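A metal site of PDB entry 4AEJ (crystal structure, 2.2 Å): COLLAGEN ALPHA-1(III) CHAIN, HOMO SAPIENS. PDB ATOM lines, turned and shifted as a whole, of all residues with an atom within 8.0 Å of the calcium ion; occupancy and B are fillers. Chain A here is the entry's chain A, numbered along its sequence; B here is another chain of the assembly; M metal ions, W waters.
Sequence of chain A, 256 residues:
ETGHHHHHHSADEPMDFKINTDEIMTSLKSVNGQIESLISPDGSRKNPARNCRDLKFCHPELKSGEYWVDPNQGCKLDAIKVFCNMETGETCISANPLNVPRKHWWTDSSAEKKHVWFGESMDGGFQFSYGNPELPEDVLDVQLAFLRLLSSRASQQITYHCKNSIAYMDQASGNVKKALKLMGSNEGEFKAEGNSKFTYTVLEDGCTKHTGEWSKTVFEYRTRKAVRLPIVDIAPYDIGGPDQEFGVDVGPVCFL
Water W1 lies within hydrogen-bond range of OD2 of Asp 78 (2.7 Å), OD2 of Asp 54 of chain B (2.9 Å) and ND2 of Asn 72 (3.4 Å).
The side-chain amide oxygen (OE1) of Gln 143 sits at hydrogen-bond distance from the backbone NH (N) of Asn 72, at 2.9 Å.
NH2 of Arg 50 of chain B lies close to ND2 of Asn 72 (3.4 Å).
O of Asp 78 sits at hydrogen-bond distance from NE2 of Gln 143.
N of Cys 75 is in hydrogen-bond range of OD2 of Asp 54 of chain B, at 3.1 Å.
SG of Cys 75 lies close to N of Leu 77 (3.5 Å).
SG of Cys 58 of chain B is disulfide-bonded to SG of Cys 75.
OD1 of Asp 70 lies close to NE2 of Gln 143.
The calcium ion is bound by O of Gln 73, OD1 of Asn 72, OD1 of Asp 78, O of Cys 75, water W1, OD1 of Asp 70 and OD2 of Asp 70.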
ATOM      1  N   PRO A  48      -0.008  10.003 -16.539  1.00  0.00           N
ATOM      2  CA  PRO A  48       0.502  11.321 -16.115  1.00  0.00           C
ATOM      3  C   PRO A  48       0.146  12.502 -17.030  1.00  0.00           C
ATOM      4  O   PRO A  48       0.031  12.333 -18.248  1.00  0.00           O
ATOM      5  CB  PRO A  48       2.022  11.114 -16.101  1.00  0.00           C
ATOM      6  CG  PRO A  48       2.260  10.010 -17.086  1.00  0.00           C
ATOM      7  CD  PRO A  48       1.077   9.077 -16.928  1.00  0.00           C
ATOM      8  N   VAL A  69       3.607  13.600 -13.237  1.00  0.00           N
ATOM      9  CA  VAL A  69       3.695  14.405 -14.440  1.00  0.00           C
ATOM     10  C   VAL A  69       4.839  13.905 -15.296  1.00  0.00           C
ATOM     11  O   VAL A  69       5.767  13.234 -14.804  1.00  0.00           O
ATOM     12  CB  VAL A  69       3.863  15.916 -14.112  1.00  0.00           C
ATOM     13  CG1 VAL A  69       2.719  16.438 -13.239  1.00  0.00           C
ATOM     14  CG2 VAL A  69       5.214  16.190 -13.454  1.00  0.00           C
ATOM     15  N   ASP A  70       4.762  14.220 -16.587  1.00  0.00           N
ATOM     16  CA  ASP A  70       5.721  13.715 -17.563  1.00  0.00           C
ATOM     17  C   ASP A  70       6.096  14.804 -18.565  1.00  0.00           C
ATOM     18  O   ASP A  70       5.594  14.812 -19.666  1.00  0.00           O
ATOM     19  CB  ASP A  70       5.113  12.530 -18.312  1.00  0.00           C
ATOM     20  CG  ASP A  70       6.131  11.747 -19.098  1.00  0.00           C
ATOM     21  OD1 ASP A  70       7.310  11.718 -18.684  1.00  0.00           O
ATOM     22  OD2 ASP A  70       5.773  11.163 -20.135  1.00  0.00           O
ATOM     23  N   PRO A  71       6.981  15.720 -18.170  1.00  0.00           N
ATOM     24  CA  PRO A  71       7.263  16.923 -18.975  1.00  0.00           C
ATOM     25  C   PRO A  71       7.812  16.582 -20.349  1.00  0.00           C
ATOM     26  O   PRO A  71       7.504  17.248 -21.323  1.00  0.00           O
ATOM     27  CB  PRO A  71       8.314  17.666 -18.158  1.00  0.00           C
ATOM     28  CG  PRO A  71       8.136  17.168 -16.739  1.00  0.00           C
ATOM     29  CD  PRO A  71       7.622  15.763 -16.838  1.00  0.00           C
ATOM     30  N   ASN A  72       8.617  15.534 -20.451  1.00  0.00           N
ATOM     31  CA  ASN A  72       9.197  15.189 -21.730  1.00  0.00           C
ATOM     32  C   ASN A  72       8.231  14.412 -22.629  1.00  0.00           C
ATOM     33  O   ASN A  72       8.553  14.122 -23.785  1.00  0.00           O
ATOM     34  CB  ASN A  72      10.555  14.493 -21.556  1.00  0.00           C
ATOM     35  CG  ASN A  72      10.437  13.090 -20.953  1.00  0.00           C
ATOM     36  OD1 ASN A  72       9.333  12.555 -20.795  1.00  0.00           O
ATOM     37  ND2 ASN A  72      11.576  12.469 -20.648  1.00  0.00           N
ATOM     38  N   GLN A  73       7.033  14.101 -22.106  1.00  0.00           N
ATOM     39  CA  GLN A  73       6.023  13.301 -22.852  1.00  0.00           C
ATOM     40  C   GLN A  73       6.620  12.004 -23.446  1.00  0.00           C
ATOM     41  O   GLN A  73       7.381  11.310 -22.767  1.00  0.00           O
ATOM     42  CB  GLN A  73       5.281  14.154 -23.902  1.00  0.00           C
ATOM     43  CG  GLN A  73       4.473  15.321 -23.337  1.00  0.00           C
ATOM     44  CD  GLN A  73       3.186  14.872 -22.652  1.00  0.00           C
ATOM     45  OE1 GLN A  73       2.107  14.861 -23.254  1.00  0.00           O
ATOM     46  NE2 GLN A  73       3.303  14.489 -21.422  1.00  0.00           N
ATOM     47  N   GLY A  74       6.296  11.661 -24.685  1.00  0.00           N
ATOM     48  CA  GLY A  74       6.750  10.380 -25.267  1.00  0.00           C
ATOM     49  C   GLY A  74       6.360   9.194 -24.391  1.00  0.00           C
ATOM     50  O   GLY A  74       5.201   9.076 -23.996  1.00  0.00           O
ATOM     51  N   CYS A  75       7.329   8.345 -24.049  1.00  0.00           N
ATOM     52  CA  CYS A  75       7.089   7.197 -23.166  1.00  0.00           C
ATOM     53  C   CYS A  75       6.647   7.617 -21.731  1.00  0.00           C
ATOM     54  O   CYS A  75       7.288   8.424 -21.063  1.00  0.00           O
ATOM     55  CB  CYS A  75       8.329   6.264 -23.115  1.00  0.00           C
ATOM     56  SG  CYS A  75       8.330   4.840 -21.964  1.00  0.00           S
ATOM     57  N   LYS A  76       5.546   7.014 -21.284  1.00  0.00           N
ATOM     58  CA  LYS A  76       4.974   7.302 -19.978  1.00  0.00           C
ATOM     59  C   LYS A  76       5.768   6.827 -18.779  1.00  0.00           C
ATOM     60  O   LYS A  76       5.525   7.294 -17.676  1.00  0.00           O
ATOM     61  CB  LYS A  76       3.539   6.796 -19.903  1.00  0.00           C
ATOM     62  CG  LYS A  76       2.575   7.877 -20.331  1.00  0.00           C
ATOM     63  CD  LYS A  76       1.255   7.345 -20.892  1.00  0.00           C
ATOM     64  CE  LYS A  76       0.627   8.399 -21.808  1.00  0.00           C
ATOM     65  NZ  LYS A  76      -0.397   7.793 -22.708  1.00  0.00           N
ATOM     66  N   LEU A  77       6.743   5.949 -18.991  1.00  0.00           N
ATOM     67  CA  LEU A  77       7.368   5.222 -17.884  1.00  0.00           C
ATOM     68  C   LEU A  77       8.393   5.994 -17.057  1.00  0.00           C
ATOM     69  O   LEU A  77       8.769   5.563 -15.972  1.00  0.00           O
ATOM     70  CB  LEU A  77       7.991   3.906 -18.398  1.00  0.00           C
ATOM     71  CG  LEU A  77       7.059   2.881 -19.054  1.00  0.00           C
ATOM     72  CD1 LEU A  77       7.841   1.642 -19.484  1.00  0.00           C
ATOM     73  CD2 LEU A  77       5.899   2.463 -18.159  1.00  0.00           C
ATOM     74  N   ASP A  78       8.859   7.137 -17.561  1.00  0.00           N
ATOM     75  CA  ASP A  78       9.818   7.917 -16.813  1.00  0.00           C
ATOM     76  C   ASP A  78       9.178   9.115 -16.128  1.00  0.00           C
ATOM     77  O   ASP A  78       9.839  10.100 -15.841  1.00  0.00           O
ATOM     78  CB  ASP A  78      10.986   8.346 -17.723  1.00  0.00           C
ATOM     79  CG  ASP A  78      10.547   9.208 -18.918  1.00  0.00           C
ATOM     80  OD1 ASP A  78       9.327   9.378 -19.158  1.00  0.00           O
ATOM     81  OD2 ASP A  78      11.432   9.714 -19.631  1.00  0.00           O
ATOM     82  N   ALA A  79       7.875   9.029 -15.887  1.00  0.00           N
ATOM     83  CA  ALA A  79       7.131  10.124 -15.266  1.00  0.00           C
ATOM     84  C   ALA A  79       7.599  10.336 -13.829  1.00  0.00           C
ATOM     85  O   ALA A  79       8.090   9.407 -13.194  1.00  0.00           O
ATOM     86  CB  ALA A  79       5.624   9.864 -15.317  1.00  0.00           C
ATOM     87  N   ILE A  80       7.480  11.575 -13.364  1.00  0.00           N
ATOM     88  CA  ILE A  80       7.928  11.930 -12.027  1.00  0.00           C
ATOM     89  C   ILE A  80       6.781  12.280 -11.074  1.00  0.00           C
ATOM     90  O   ILE A  80       5.688  12.700 -11.490  1.00  0.00           O
ATOM     91  CB  ILE A  80       8.988  13.054 -12.051  1.00  0.00           C
ATOM     92  CG1 ILE A  80       8.446  14.282 -12.787  1.00  0.00           C
ATOM     93  CG2 ILE A  80      10.281  12.551 -12.699  1.00  0.00           C
ATOM     94  CD1 ILE A  80       9.188  15.570 -12.506  1.00  0.00           C
ATOM     95  N   VAL A 139      17.895  10.595 -17.191  1.00  0.00           N
ATOM     96  CA  VAL A 139      16.449  10.696 -17.390  1.00  0.00           C
ATOM     97  C   VAL A 139      15.872  11.843 -16.550  1.00  0.00           C
ATOM     98  O   VAL A 139      15.025  12.614 -17.032  1.00  0.00           O
ATOM     99  CB  VAL A 139      15.784   9.333 -17.076  1.00  0.00           C
ATOM    100  CG1 VAL A 139      14.291   9.445 -16.824  1.00  0.00           C
ATOM    101  CG2 VAL A 139      16.076   8.353 -18.195  1.00  0.00           C
ATOM    102  N   VAL A 142      16.826  15.177 -17.997  1.00  0.00           N
ATOM    103  CA  VAL A 142      15.932  15.510 -19.098  1.00  0.00           C
ATOM    104  C   VAL A 142      14.565  16.013 -18.609  1.00  0.00           C
ATOM    105  O   VAL A 142      14.029  16.978 -19.141  1.00  0.00           O
ATOM    106  CB  VAL A 142      15.775  14.334 -20.085  1.00  0.00           C
ATOM    107  CG1 VAL A 142      14.693  14.635 -21.112  1.00  0.00           C
ATOM    108  CG2 VAL A 142      17.095  14.055 -20.774  1.00  0.00           C
ATOM    109  N   GLN A 143      14.003  15.365 -17.593  1.00  0.00           N
ATOM    110  CA  GLN A 143      12.703  15.808 -17.120  1.00  0.00           C
ATOM    111  C   GLN A 143      12.835  17.224 -16.570  1.00  0.00           C
ATOM    112  O   GLN A 143      12.016  18.093 -16.891  1.00  0.00           O
ATOM    113  CB  GLN A 143      12.090  14.845 -16.106  1.00  0.00           C
ATOM    114  CG  GLN A 143      11.683  13.494 -16.726  1.00  0.00           C
ATOM    115  CD  GLN A 143      10.383  13.541 -17.526  1.00  0.00           C
ATOM    116  OE1 GLN A 143      10.130  14.489 -18.262  1.00  0.00           O
ATOM    117  NE2 GLN A 143       9.555  12.494 -17.382  1.00  0.00           N
ATOM    118  N   PHE A 146      13.277  19.906 -19.402  1.00  0.00           N
ATOM    119  CA  PHE A 146      11.997  20.288 -20.008  1.00  0.00           C
ATOM    120  C   PHE A 146      11.306  21.378 -19.188  1.00  0.00           C
ATOM    121  O   PHE A 146      10.780  22.330 -19.738  1.00  0.00           O
ATOM    122  CB  PHE A 146      11.077  19.048 -20.214  1.00  0.00           C
ATOM    123  CG  PHE A 146      11.199  18.423 -21.597  1.00  0.00           C
ATOM    124  CD1 PHE A 146      12.202  17.462 -21.862  1.00  0.00           C
ATOM    125  CD2 PHE A 146      10.355  18.812 -22.643  1.00  0.00           C
ATOM    126  CE1 PHE A 146      12.332  16.890 -23.131  1.00  0.00           C
ATOM    127  CE2 PHE A 146      10.489  18.258 -23.909  1.00  0.00           C
ATOM    128  CZ  PHE A 146      11.474  17.285 -24.151  1.00  0.00           C
ATOM    129  N   ARG B  50      10.149   8.958 -29.510  1.00  0.00           N
ATOM    130  CA  ARG B  50      10.587  10.329 -29.311  1.00  0.00           C
ATOM    131  C   ARG B  50      12.113  10.432 -29.527  1.00  0.00           C
ATOM    132  O   ARG B  50      12.602  11.342 -30.191  1.00  0.00           O
ATOM    133  CB  ARG B  50      10.216  10.796 -27.901  1.00  0.00           C
ATOM    134  CG  ARG B  50      10.599  12.245 -27.585  1.00  0.00           C
ATOM    135  CD  ARG B  50      10.118  12.660 -26.202  1.00  0.00           C
ATOM    136  NE  ARG B  50      10.939  12.073 -25.134  1.00  0.00           N
ATOM    137  CZ  ARG B  50      12.107  12.566 -24.706  1.00  0.00           C
ATOM    138  NH1 ARG B  50      12.633  13.687 -25.225  1.00  0.00           N
ATOM    139  NH2 ARG B  50      12.760  11.940 -23.737  1.00  0.00           N
ATOM    140  N   ASP B  54      13.947   6.901 -24.853  1.00  0.00           N
ATOM    141  CA  ASP B  54      12.554   6.506 -24.656  1.00  0.00           C
ATOM    142  C   ASP B  54      12.311   5.108 -25.150  1.00  0.00           C
ATOM    143  O   ASP B  54      11.611   4.333 -24.508  1.00  0.00           O
ATOM    144  CB  ASP B  54      11.604   7.462 -25.382  1.00  0.00           C
ATOM    145  CG  ASP B  54      11.288   8.682 -24.576  1.00  0.00           C
ATOM    146  OD1 ASP B  54      12.161   9.089 -23.758  1.00  0.00           O
ATOM    147  OD2 ASP B  54      10.192   9.229 -24.755  1.00  0.00           O
ATOM    148  N   PHE B  57      13.681   2.638 -22.772  1.00  0.00           N
ATOM    149  CA  PHE B  57      12.915   2.561 -21.509  1.00  0.00           C
ATOM    150  C   PHE B  57      11.677   1.713 -21.707  1.00  0.00           C
ATOM    151  O   PHE B  57      11.392   0.829 -20.894  1.00  0.00           O
ATOM    152  CB  PHE B  57      12.468   3.956 -21.037  1.00  0.00           C
ATOM    153  CG  PHE B  57      12.488   4.138 -19.541  1.00  0.00           C
ATOM    154  CD1 PHE B  57      11.478   3.616 -18.752  1.00  0.00           C
ATOM    155  CD2 PHE B  57      13.509   4.853 -18.926  1.00  0.00           C
ATOM    156  CE1 PHE B  57      11.496   3.779 -17.368  1.00  0.00           C
ATOM    157  CE2 PHE B  57      13.537   5.025 -17.542  1.00  0.00           C
ATOM    158  CZ  PHE B  57      12.524   4.475 -16.763  1.00  0.00           C
ATOM    159  N   CYS B  58      10.968   1.998 -22.782  1.00  0.00           N
ATOM    160  CA  CYS B  58       9.689   1.384 -23.115  1.00  0.00           C
ATOM    161  C   CYS B  58       9.809   0.035 -23.873  1.00  0.00           C
ATOM    162  O   CYS B  58       8.860  -0.743 -23.943  1.00  0.00           O
ATOM    163  CB  CYS B  58       8.856   2.406 -23.923  1.00  0.00           C
ATOM    164  SG  CYS B  58       7.519   3.275 -23.019  1.00  0.00           S
HETATM  165 CA    CA M   1       8.114  10.578 -20.735  1.00  0.00          CA
HETATM  166  O   HOH W   1      10.022   9.674 -21.910  1.00  0.00           O
